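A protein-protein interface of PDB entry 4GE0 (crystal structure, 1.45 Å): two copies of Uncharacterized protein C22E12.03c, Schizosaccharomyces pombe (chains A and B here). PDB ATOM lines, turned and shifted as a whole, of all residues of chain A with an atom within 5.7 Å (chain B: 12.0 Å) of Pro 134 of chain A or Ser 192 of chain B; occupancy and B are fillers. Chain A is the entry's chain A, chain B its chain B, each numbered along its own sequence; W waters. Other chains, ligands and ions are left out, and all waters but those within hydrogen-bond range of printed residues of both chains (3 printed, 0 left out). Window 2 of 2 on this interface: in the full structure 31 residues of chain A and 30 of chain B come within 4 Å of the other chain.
NE2 of His 133 of chain A sits at hydrogen-bond distance from O of Ser 190 of chain B (2.9 Å).
N of Gly 165 of chain A sits at hydrogen-bond distance from O of Leu 191 of chain B, at 2.8 Å.
The backbone nitrogen of Pro 164 of chain A lies close to the backbone carbonyl oxygen of Leu 191 of chain B (3.5 Å).
Water W3 lies within hydrogen-bond range of the side-chain amide oxygen of Gln 162 of chain A (2.7 Å) and the backbone carbonyl oxygen of Ser 192 of chain B (2.9 Å).
Water W2 lies within hydrogen-bond range of O of Lys 189 of chain B (2.7 Å), OG of Ser 192 of chain B (2.8 Å), NE2 of His 133 of chain A (3.2 Å) and O of Ser 190 of chain B (3.5 Å).
Water W1 bridges the backbone carbonyl oxygen of Gly 165 of chain A (2.8 Å) and the side-chain sulfur of Met 193 of chain B (3.7 Å).
1 position is printed for both chains.
Of the 11 pairs that touch across the chains among the printed residues, none has its exchanged pair printed and touching as well.
Of the printed residues of chain A, Ser 192 of chain B touches Pro 134 (3.3 Å), Gln 162 (3.9 Å), Gly 165 (3.99 Å) and Thr 166 (3.2 Å).
No residue of chain B comes within 4 Å of Gly 132 of chain A.
His 133 of chain A touches one residue of chain B.
Gln 162 of chain A touches just one residue of chain B: Ser 192.
Gly 163 of chain A touches just one residue of chain B: Leu 191.
Printed residues of chain B within 4 Å of Pro 164 of chain A: Arg 29 (3.4 Å) and Leu 191 (3.4 Å).
Printed residues of chain B within 4 Å of Gly 165 of chain A: Leu 191 (2.8 Å), Ser 192 (3.99 Å), Met 193 (3.8 Å) and Pro 194 (3.3 Å).
Of the printed residues of chain A, Pro 194 of chain B touches Gly 165 (3.3 Å).
Of the printed residues of chain A, Arg 29 of chain B touches Pro 164.
The nearest residue of chain B that does not touch Pro 134 of chain A is Lys 189 of chain B (5.8 Å).
The nearest printed residue of chain A that does not touch Ser 192 of chain B is His 133 of chain A (4.1 Å).
The side-chain hydroxyl (OG) of Ser 135 of chain A is in hydrogen-bond range of a ring nitrogen (ND1) of His 133 of chain A (2.9 Å).
The backbone NH (N) of His 133 of chain A lies close to the backbone carbonyl oxygen (O) of Gln 162 of chain A, at 3.1 Å.
OH of Tyr 147 of chain A lies within hydrogen-bond range of NE2 of Gln 162 of chain A.
N of Gly 163 of chain A sits at hydrogen-bond distance from OG1 of Thr 166 of chain A.
NH1 of Arg 29 of chain B lies within hydrogen-bond range of O of Gly 25 of chain B (3.0 Å).
The side-chain hydroxyl of Ser 190 of chain B lies within hydrogen-bond range of the backbone carbonyl oxygen of Val 187 of chain B, 2.6 Å away.
Among the printed residues, merely in contact across the chains: Thr 166 of chain A with Ser 192 of chain B, Gly 165 of chain A with Pro 194 of chain B, Pro 134 of chain A with Ser 192 of chain B, Pro 164 of chain A with Arg 29 of chain B, Gly 163 of chain A with Leu 191 of chain B, Gly 165 of chain A with Met 193 of chain B, Gln 162 of chain A with Ser 192 of chain B and Gly 165 of chain A with Ser 192 of chain B.
Of the 13 printed residues of chain A, 7 touch a printed residue of chain B.
Hydrophobic or aromatic side chains of chain A within 4 Å of the printed part of chain B: His 133, Pro 134 and Pro 164.
Printed residues of chain B that touch a printed residue of chain A: Arg 29, Ser 190, Leu 191, Ser 192, Met 193 and Pro 194.
Among the printed residues, no Asp or Glu carboxylate lies within 4 Å of a Lys or Arg side-chain nitrogen of the other chain.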
ATOM      1  N   GLY A 132     -17.762   5.279 -25.963  1.00  0.00           N
ATOM      2  CA  GLY A 132     -18.314   6.256 -26.893  1.00  0.00           C
ATOM      3  C   GLY A 132     -19.804   6.016 -27.032  1.00  0.00           C
ATOM      4  O   GLY A 132     -20.383   5.176 -26.333  1.00  0.00           O
ATOM      5  N   HIS A 133     -20.445   6.806 -27.879  1.00  0.00           N
ATOM      6  CA  HIS A 133     -21.885   6.650 -28.042  1.00  0.00           C
ATOM      7  C   HIS A 133     -22.213   5.255 -28.575  1.00  0.00           C
ATOM      8  O   HIS A 133     -21.496   4.744 -29.419  1.00  0.00           O
ATOM      9  CB  HIS A 133     -22.453   7.730 -28.964  1.00  0.00           C
ATOM     10  CG  HIS A 133     -23.921   7.934 -28.784  1.00  0.00           C
ATOM     11  ND1 HIS A 133     -24.852   7.277 -29.556  1.00  0.00           N
ATOM     12  CD2 HIS A 133     -24.616   8.533 -27.788  1.00  0.00           C
ATOM     13  CE1 HIS A 133     -26.065   7.527 -29.090  1.00  0.00           C
ATOM     14  NE2 HIS A 133     -25.948   8.311 -28.034  1.00  0.00           N
ATOM     15  N   PRO A 134     -23.317   4.643 -28.100  1.00  0.00           N
ATOM     16  CA  PRO A 134     -23.680   3.314 -28.591  1.00  0.00           C
ATOM     17  C   PRO A 134     -23.820   3.301 -30.104  1.00  0.00           C
ATOM     18  O   PRO A 134     -23.580   2.253 -30.724  1.00  0.00           O
ATOM     19  CB  PRO A 134     -25.028   3.052 -27.912  1.00  0.00           C
ATOM     20  CG  PRO A 134     -24.865   3.741 -26.583  1.00  0.00           C
ATOM     21  CD  PRO A 134     -24.081   5.017 -26.891  1.00  0.00           C
ATOM     22  N   SER A 135     -24.153   4.457 -30.684  1.00  0.00           N
ATOM     23  CA  SER A 135     -24.380   4.598 -32.125  1.00  0.00           C
ATOM     24  C   SER A 135     -23.096   4.390 -32.920  1.00  0.00           C
ATOM     25  O   SER A 135     -23.143   4.051 -34.102  1.00  0.00           O
ATOM     26  CB  SER A 135     -24.975   5.977 -32.454  1.00  0.00           C
ATOM     27  OG  SER A 135     -24.034   7.023 -32.299  1.00  0.00           O
ATOM     28  N   VAL A 136     -21.957   4.610 -32.272  1.00  0.00           N
ATOM     29  CA  VAL A 136     -20.658   4.445 -32.922  1.00  0.00           C
ATOM     30  C   VAL A 136     -19.884   3.250 -32.388  1.00  0.00           C
ATOM     31  O   VAL A 136     -18.704   3.088 -32.689  1.00  0.00           O
ATOM     32  CB  VAL A 136     -19.776   5.730 -32.892  1.00  0.00           C
ATOM     33  CG1 VAL A 136     -20.472   6.878 -33.624  1.00  0.00           C
ATOM     34  CG2 VAL A 136     -19.425   6.161 -31.454  1.00  0.00           C
ATOM     35  N   ARG A 137     -20.537   2.416 -31.589  1.00  0.00           N
ATOM     36  CA  ARG A 137     -19.837   1.307 -30.959  1.00  0.00           C
ATOM     37  C   ARG A 137     -19.154   0.421 -32.011  1.00  0.00           C
ATOM     38  O   ARG A 137     -17.978   0.084 -31.880  1.00  0.00           O
ATOM     39  CB  ARG A 137     -20.788   0.471 -30.099  1.00  0.00           C
ATOM     40  CG  ARG A 137     -20.108  -0.766 -29.539  1.00  0.00           C
ATOM     41  CD  ARG A 137     -20.975  -1.494 -28.549  1.00  0.00           C
ATOM     42  NE  ARG A 137     -20.304  -2.679 -28.031  1.00  0.00           N
ATOM     43  CZ  ARG A 137     -20.687  -3.330 -26.940  1.00  0.00           C
ATOM     44  NH1 ARG A 137     -21.747  -2.914 -26.252  1.00  0.00           N
ATOM     45  NH2 ARG A 137     -20.011  -4.389 -26.532  1.00  0.00           N
ATOM     46  N   GLY A 138     -19.901   0.028 -33.041  1.00  0.00           N
ATOM     47  CA  GLY A 138     -19.330  -0.750 -34.141  1.00  0.00           C
ATOM     48  C   GLY A 138     -18.097  -0.114 -34.770  1.00  0.00           C
ATOM     49  O   GLY A 138     -17.089  -0.790 -34.998  1.00  0.00           O
ATOM     50  N   TYR A 147     -14.708  -2.162 -26.583  1.00  0.00           N
ATOM     51  CA  TYR A 147     -15.695  -1.213 -26.101  1.00  0.00           C
ATOM     52  C   TYR A 147     -16.177  -1.591 -24.703  1.00  0.00           C
ATOM     53  O   TYR A 147     -16.564  -2.740 -24.462  1.00  0.00           O
ATOM     54  CB  TYR A 147     -16.870  -1.147 -27.076  1.00  0.00           C
ATOM     55  CG  TYR A 147     -17.944  -0.145 -26.707  1.00  0.00           C
ATOM     56  CD1 TYR A 147     -18.992  -0.495 -25.855  1.00  0.00           C
ATOM     57  CD2 TYR A 147     -17.936   1.144 -27.244  1.00  0.00           C
ATOM     58  CE1 TYR A 147     -19.991   0.420 -25.530  1.00  0.00           C
ATOM     59  CE2 TYR A 147     -18.936   2.060 -26.931  1.00  0.00           C
ATOM     60  CZ  TYR A 147     -19.946   1.697 -26.064  1.00  0.00           C
ATOM     61  OH  TYR A 147     -20.929   2.591 -25.741  1.00  0.00           O
ATOM     62  N   GLN A 162     -19.523   8.386 -22.978  1.00  0.00           N
ATOM     63  CA  GLN A 162     -20.588   7.835 -23.854  1.00  0.00           C
ATOM     64  C   GLN A 162     -21.454   8.862 -24.595  1.00  0.00           C
ATOM     65  O   GLN A 162     -21.767   8.683 -25.780  1.00  0.00           O
ATOM     66  CB  GLN A 162     -21.482   6.852 -23.096  1.00  0.00           C
ATOM     67  CG  GLN A 162     -20.749   5.570 -22.745  1.00  0.00           C
ATOM     68  CD  GLN A 162     -21.679   4.502 -22.195  1.00  0.00           C
ATOM     69  OE1 GLN A 162     -22.398   4.734 -21.221  1.00  0.00           O
ATOM     70  NE2 GLN A 162     -21.675   3.325 -22.819  1.00  0.00           N
ATOM     71  N   GLY A 163     -21.991   9.839 -23.882  1.00  0.00           N
ATOM     72  CA  GLY A 163     -23.054  10.635 -24.483  1.00  0.00           C
ATOM     73  C   GLY A 163     -23.412  11.879 -23.702  1.00  0.00           C
ATOM     74  O   GLY A 163     -22.721  12.251 -22.758  1.00  0.00           O
ATOM     75  N   PRO A 164     -24.411  12.613 -24.185  1.00  0.00           N
ATOM     76  CA  PRO A 164     -24.727  13.863 -23.499  1.00  0.00           C
ATOM     77  C   PRO A 164     -25.019  13.625 -22.017  1.00  0.00           C
ATOM     78  O   PRO A 164     -24.631  14.445 -21.175  1.00  0.00           O
ATOM     79  CB  PRO A 164     -25.973  14.370 -24.219  1.00  0.00           C
ATOM     80  CG  PRO A 164     -26.184  13.499 -25.392  1.00  0.00           C
ATOM     81  CD  PRO A 164     -25.318  12.296 -25.301  1.00  0.00           C
ATOM     82  N   GLY A 165     -25.656  12.503 -21.697  1.00  0.00           N
ATOM     83  CA  GLY A 165     -25.947  12.132 -20.313  1.00  0.00           C
ATOM     84  C   GLY A 165     -24.714  11.966 -19.441  1.00  0.00           C
ATOM     85  O   GLY A 165     -24.810  12.047 -18.213  1.00  0.00           O
ATOM     86  N   THR A 166     -23.562  11.705 -20.059  1.00  0.00           N
ATOM     87  CA  THR A 166     -22.349  11.464 -19.294  1.00  0.00           C
ATOM     88  C   THR A 166     -21.369  12.630 -19.370  1.00  0.00           C
ATOM     89  O   THR A 166     -20.237  12.510 -18.894  1.00  0.00           O
ATOM     90  CB  THR A 166     -21.619  10.155 -19.721  1.00  0.00           C
ATOM     91  OG1 THR A 166     -21.126  10.272 -21.063  1.00  0.00           O
ATOM     92  CG2 THR A 166     -22.549   8.963 -19.622  1.00  0.00           C
ATOM     93  N   ALA B  22     -28.788  21.668 -21.551  1.00  0.00           N
ATOM     94  CA  ALA B  22     -29.460  20.402 -21.308  1.00  0.00           C
ATOM     95  C   ALA B  22     -30.903  20.404 -21.832  1.00  0.00           C
ATOM     96  O   ALA B  22     -31.268  19.580 -22.706  1.00  0.00           O
ATOM     97  CB  ALA B  22     -29.357  20.004 -19.834  1.00  0.00           C
ATOM     98  N   GLY B  25     -30.902  20.766 -25.716  1.00  0.00           N
ATOM     99  CA  GLY B  25     -30.538  19.585 -26.486  1.00  0.00           C
ATOM    100  C   GLY B  25     -31.572  18.492 -26.375  1.00  0.00           C
ATOM    101  O   GLY B  25     -31.786  17.727 -27.310  1.00  0.00           O
ATOM    102  N   ILE B  26     -32.247  18.413 -25.234  1.00  0.00           N
ATOM    103  CA  ILE B  26     -33.265  17.385 -25.040  1.00  0.00           C
ATOM    104  C   ILE B  26     -34.502  17.656 -25.899  1.00  0.00           C
ATOM    105  O   ILE B  26     -34.997  16.776 -26.603  1.00  0.00           O
ATOM    106  CB  ILE B  26     -33.600  17.231 -23.537  1.00  0.00           C
ATOM    107  CG1 ILE B  26     -32.417  16.563 -22.819  1.00  0.00           C
ATOM    108  CG2 ILE B  26     -34.904  16.445 -23.324  1.00  0.00           C
ATOM    109  CD1 ILE B  26     -32.421  16.722 -21.302  1.00  0.00           C
ATOM    110  N   ARG B  29     -33.728  17.110 -29.610  1.00  0.00           N
ATOM    111  CA  ARG B  29     -33.731  15.685 -29.950  1.00  0.00           C
ATOM    112  C   ARG B  29     -35.154  15.145 -30.060  1.00  0.00           C
ATOM    113  O   ARG B  29     -35.424  14.247 -30.862  1.00  0.00           O
ATOM    114  CB  ARG B  29     -32.956  14.907 -28.893  1.00  0.00           C
ATOM    115  CG  ARG B  29     -31.460  14.952 -29.104  1.00  0.00           C
ATOM    116  CD  ARG B  29     -30.727  14.483 -27.847  1.00  0.00           C
ATOM    117  NE  ARG B  29     -29.268  14.446 -27.970  1.00  0.00           N
ATOM    118  CZ  ARG B  29     -28.473  15.509 -27.913  1.00  0.00           C
ATOM    119  NH1 ARG B  29     -28.978  16.716 -27.699  1.00  0.00           N
ATOM    120  NH2 ARG B  29     -27.171  15.355 -28.047  1.00  0.00           N
ATOM    121  N   GLY B 165     -25.387  19.748 -12.234  1.00  0.00           N
ATOM    122  CA  GLY B 165     -25.382  18.290 -12.183  1.00  0.00           C
ATOM    123  C   GLY B 165     -26.740  17.641 -12.456  1.00  0.00           C
ATOM    124  O   GLY B 165     -26.794  16.470 -12.843  1.00  0.00           O
ATOM    125  N   MET B 168     -29.691  17.667 -16.844  1.00  0.00           N
ATOM    126  CA  MET B 168     -30.261  16.618 -17.681  1.00  0.00           C
ATOM    127  C   MET B 168     -31.537  16.004 -17.108  1.00  0.00           C
ATOM    128  O   MET B 168     -32.529  15.816 -17.831  1.00  0.00           O
ATOM    129  CB  MET B 168     -29.213  15.556 -17.991  1.00  0.00           C
ATOM    130  CG  MET B 168     -28.050  16.072 -18.865  1.00  0.00           C
ATOM    131  SD  MET B 168     -28.497  16.566 -20.557  1.00  0.00           S
ATOM    132  CE  MET B 168     -28.808  14.964 -21.306  1.00  0.00           C
ATOM    133  N   LEU B 169     -31.518  15.660 -15.827  1.00  0.00           N
ATOM    134  CA  LEU B 169     -32.728  15.112 -15.178  1.00  0.00           C
ATOM    135  C   LEU B 169     -33.891  16.118 -15.196  1.00  0.00           C
ATOM    136  O   LEU B 169     -35.047  15.761 -15.380  1.00  0.00           O
ATOM    137  CB  LEU B 169     -32.437  14.701 -13.732  1.00  0.00           C
ATOM    138  CG  LEU B 169     -31.476  13.517 -13.563  1.00  0.00           C
ATOM    139  CD1 LEU B 169     -31.098  13.417 -12.106  1.00  0.00           C
ATOM    140  CD2 LEU B 169     -32.121  12.229 -14.069  1.00  0.00           C
ATOM    141  N   LEU B 172     -35.296  16.262 -18.780  1.00  0.00           N
ATOM    142  CA  LEU B 172     -36.092  15.061 -19.000  1.00  0.00           C
ATOM    143  C   LEU B 172     -37.453  15.143 -18.315  1.00  0.00           C
ATOM    144  O   LEU B 172     -38.463  14.702 -18.865  1.00  0.00           O
ATOM    145  CB  LEU B 172     -35.309  13.812 -18.557  1.00  0.00           C
ATOM    146  CG  LEU B 172     -34.205  13.372 -19.520  1.00  0.00           C
ATOM    147  CD1 LEU B 172     -33.277  12.424 -18.796  1.00  0.00           C
ATOM    148  CD2 LEU B 172     -34.816  12.717 -20.768  1.00  0.00           C
ATOM    149  N   LEU B 175     -39.648  17.214 -20.497  1.00  0.00           N
ATOM    150  CA  LEU B 175     -40.036  16.449 -21.671  1.00  0.00           C
ATOM    151  C   LEU B 175     -41.112  15.418 -21.318  1.00  0.00           C
ATOM    152  O   LEU B 175     -42.005  15.155 -22.106  1.00  0.00           O
ATOM    153  CB  LEU B 175     -38.787  15.753 -22.254  1.00  0.00           C
ATOM    154  CG  LEU B 175     -39.045  14.907 -23.508  1.00  0.00           C
ATOM    155  CD1 LEU B 175     -39.532  15.771 -24.697  1.00  0.00           C
ATOM    156  CD2 LEU B 175     -37.796  14.117 -23.879  1.00  0.00           C
ATOM    157  N   LYS B 183     -41.758   8.489 -27.630  1.00  0.00           N
ATOM    158  CA  LYS B 183     -40.835   9.602 -27.869  1.00  0.00           C
ATOM    159  C   LYS B 183     -39.932   9.823 -26.663  1.00  0.00           C
ATOM    160  O   LYS B 183     -38.713   9.947 -26.795  1.00  0.00           O
ATOM    161  CB  LYS B 183     -41.597  10.886 -28.223  1.00  0.00           C
ATOM    162  CG  LYS B 183     -40.690  12.096 -28.434  1.00  0.00           C
ATOM    163  CD  LYS B 183     -39.840  11.961 -29.690  1.00  0.00           C
ATOM    164  CE  LYS B 183     -40.658  12.204 -30.964  1.00  0.00           C
ATOM    165  NZ  LYS B 183     -41.348  13.526 -30.994  1.00  0.00           N
ATOM    166  N   TYR B 184     -40.519   9.823 -25.475  1.00  0.00           N
ATOM    167  CA  TYR B 184     -39.714   9.989 -24.266  1.00  0.00           C
ATOM    168  C   TYR B 184     -38.665   8.870 -24.135  1.00  0.00           C
ATOM    169  O   TYR B 184     -37.480   9.146 -23.937  1.00  0.00           O
ATOM    170  CB  TYR B 184     -40.620  10.026 -23.026  1.00  0.00           C
ATOM    171  CG  TYR B 184     -39.835  10.214 -21.759  1.00  0.00           C
ATOM    172  CD1 TYR B 184     -39.492  11.486 -21.320  1.00  0.00           C
ATOM    173  CD2 TYR B 184     -39.367   9.115 -21.035  1.00  0.00           C
ATOM    174  CE1 TYR B 184     -38.694  11.659 -20.199  1.00  0.00           C
ATOM    175  CE2 TYR B 184     -38.535   9.286 -19.937  1.00  0.00           C
ATOM    176  CZ  TYR B 184     -38.251  10.557 -19.498  1.00  0.00           C
ATOM    177  OH  TYR B 184     -37.418  10.752 -18.410  1.00  0.00           O
ATOM    178  N   ASN B 185     -39.091   7.615 -24.283  1.00  0.00           N
ATOM    179  CA  ASN B 185     -38.157   6.497 -24.182  1.00  0.00           C
ATOM    180  C   ASN B 185     -37.031   6.544 -25.204  1.00  0.00           C
ATOM    181  O   ASN B 185     -35.869   6.305 -24.857  1.00  0.00           O
ATOM    182  CB  ASN B 185     -38.900   5.165 -24.283  1.00  0.00           C
ATOM    183  CG  ASN B 185     -39.755   4.890 -23.063  1.00  0.00           C
ATOM    184  OD1 ASN B 185     -39.560   5.513 -22.013  1.00  0.00           O
ATOM    185  ND2 ASN B 185     -40.721   3.993 -23.198  1.00  0.00           N
ATOM    186  N   ALA B 186     -37.355   6.963 -26.430  1.00  0.00           N
ATOM    187  CA  ALA B 186     -36.333   7.075 -27.479  1.00  0.00           C
ATOM    188  C   ALA B 186     -35.331   8.184 -27.205  1.00  0.00           C
ATOM    189  O   ALA B 186     -34.126   7.974 -27.284  1.00  0.00           O
ATOM    190  CB  ALA B 186     -36.979   7.251 -28.856  1.00  0.00           C
ATOM    191  N   VAL B 187     -35.823   9.359 -26.826  1.00  0.00           N
ATOM    192  CA  VAL B 187     -34.929  10.440 -26.454  1.00  0.00           C
ATOM    193  C   VAL B 187     -34.061  10.052 -25.249  1.00  0.00           C
ATOM    194  O   VAL B 187     -32.841  10.200 -25.276  1.00  0.00           O
ATOM    195  CB  VAL B 187     -35.692  11.771 -26.201  1.00  0.00           C
ATOM    196  CG1 VAL B 187     -34.729  12.811 -25.696  1.00  0.00           C
ATOM    197  CG2 VAL B 187     -36.342  12.256 -27.495  1.00  0.00           C
ATOM    198  N   TYR B 188     -34.690   9.476 -24.227  1.00  0.00           N
ATOM    199  CA  TYR B 188     -33.946   9.041 -23.043  1.00  0.00           C
ATOM    200  C   TYR B 188     -32.800   8.096 -23.414  1.00  0.00           C
ATOM    201  O   TYR B 188     -31.641   8.322 -23.045  1.00  0.00           O
ATOM    202  CB  TYR B 188     -34.886   8.366 -22.047  1.00  0.00           C
ATOM    203  CG  TYR B 188     -34.206   7.951 -20.760  1.00  0.00           C
ATOM    204  CD1 TYR B 188     -33.528   6.728 -20.673  1.00  0.00           C
ATOM    205  CD2 TYR B 188     -34.153   8.809 -19.665  1.00  0.00           C
ATOM    206  CE1 TYR B 188     -32.864   6.357 -19.518  1.00  0.00           C
ATOM    207  CE2 TYR B 188     -33.476   8.440 -18.498  1.00  0.00           C
ATOM    208  CZ  TYR B 188     -32.826   7.224 -18.439  1.00  0.00           C
ATOM    209  OH  TYR B 188     -32.170   6.810 -17.282  1.00  0.00           O
ATOM    210  N   LYS B 189     -33.134   7.069 -24.196  1.00  0.00           N
ATOM    211  CA  LYS B 189     -32.145   6.058 -24.588  1.00  0.00           C
ATOM    212  C   LYS B 189     -30.976   6.669 -25.351  1.00  0.00           C
ATOM    213  O   LYS B 189     -29.820   6.280 -25.140  1.00  0.00           O
ATOM    214  CB  LYS B 189     -32.815   4.971 -25.432  1.00  0.00           C
ATOM    215  CG  LYS B 189     -31.932   3.769 -25.720  1.00  0.00           C
ATOM    216  CD  LYS B 189     -32.703   2.766 -26.555  1.00  0.00           C
ATOM    217  CE  LYS B 189     -33.429   1.747 -25.682  1.00  0.00           C
ATOM    218  NZ  LYS B 189     -34.469   2.368 -24.816  1.00  0.00           N
ATOM    219  N   SER B 190     -31.259   7.703 -26.143  1.00  0.00           N
ATOM    220  CA  SER B 190     -30.233   8.351 -26.967  1.00  0.00           C
ATOM    221  C   SER B 190     -29.209   9.136 -26.156  1.00  0.00           C
ATOM    222  O   SER B 190     -28.152   9.489 -26.660  1.00  0.00           O
ATOM    223  CB  SER B 190     -30.885   9.285 -27.998  1.00  0.00           C
ATOM    224  OG  SER B 190     -31.292  10.513 -27.403  1.00  0.00           O
ATOM    225  N   LEU B 191     -29.531   9.443 -24.906  1.00  0.00           N
ATOM    226  CA  LEU B 191     -28.659  10.296 -24.099  1.00  0.00           C
ATOM    227  C   LEU B 191     -27.530   9.552 -23.399  1.00  0.00           C
ATOM    228  O   LEU B 191     -26.556  10.165 -22.961  1.00  0.00           O
ATOM    229  CB  LEU B 191     -29.481  11.079 -23.075  1.00  0.00           C
ATOM    230  CG  LEU B 191     -30.618  11.936 -23.616  1.00  0.00           C
ATOM    231  CD1 LEU B 191     -31.469  12.485 -22.461  1.00  0.00           C
ATOM    232  CD2 LEU B 191     -30.103  13.079 -24.490  1.00  0.00           C
ATOM    233  N   SER B 192     -27.655   8.237 -23.264  1.00  0.00           N
ATOM    234  CA  SER B 192     -26.702   7.442 -22.477  1.00  0.00           C
ATOM    235  C   SER B 192     -26.638   7.912 -21.031  1.00  0.00           C
ATOM    236  O   SER B 192     -25.567   8.166 -20.476  1.00  0.00           O
ATOM    237  CB  SER B 192     -25.312   7.416 -23.131  1.00  0.00           C
ATOM    238  OG  SER B 192     -25.337   6.521 -24.234  1.00  0.00           O
ATOM    239  N   MET B 193     -27.808   8.043 -20.420  1.00  0.00           N
ATOM    240  CA  MET B 193     -27.879   8.440 -19.030  1.00  0.00           C
ATOM    241  C   MET B 193     -27.158   7.430 -18.149  1.00  0.00           C
ATOM    242  O   MET B 193     -27.321   6.219 -18.333  1.00  0.00           O
ATOM    243  CB  MET B 193     -29.340   8.587 -18.611  1.00  0.00           C
ATOM    244  CG  MET B 193     -30.095   9.698 -19.370  1.00  0.00           C
ATOM    245  SD  MET B 193     -29.446  11.350 -19.024  1.00  0.00           S
ATOM    246  CE  MET B 193     -30.046  11.583 -17.338  1.00  0.00           C
ATOM    247  N   PRO B 194     -26.379   7.917 -17.169  1.00  0.00           N
ATOM    248  CA  PRO B 194     -25.543   7.008 -16.375  1.00  0.00           C
ATOM    249  C   PRO B 194     -26.357   6.239 -15.352  1.00  0.00           C
ATOM    250  O   PRO B 194     -27.463   6.653 -14.999  1.00  0.00           O
ATOM    251  CB  PRO B 194     -24.555   7.949 -15.678  1.00  0.00           C
ATOM    252  CG  PRO B 194     -25.262   9.252 -15.619  1.00  0.00           C
ATOM    253  CD  PRO B 194     -26.093   9.332 -16.876  1.00  0.00           C
ATOM    254  OXT PRO B 194     -25.929   5.179 -14.879  1.00  0.00           O
HETATM  255  O   HOH W   1     -27.065  13.221 -16.975  1.00  0.00           O
HETATM  256  O   HOH W   2     -27.313   6.145 -26.120  1.00  0.00           O
HETATM  257  O   HOH W   3     -23.970   5.942 -19.400  1.00  0.00           O
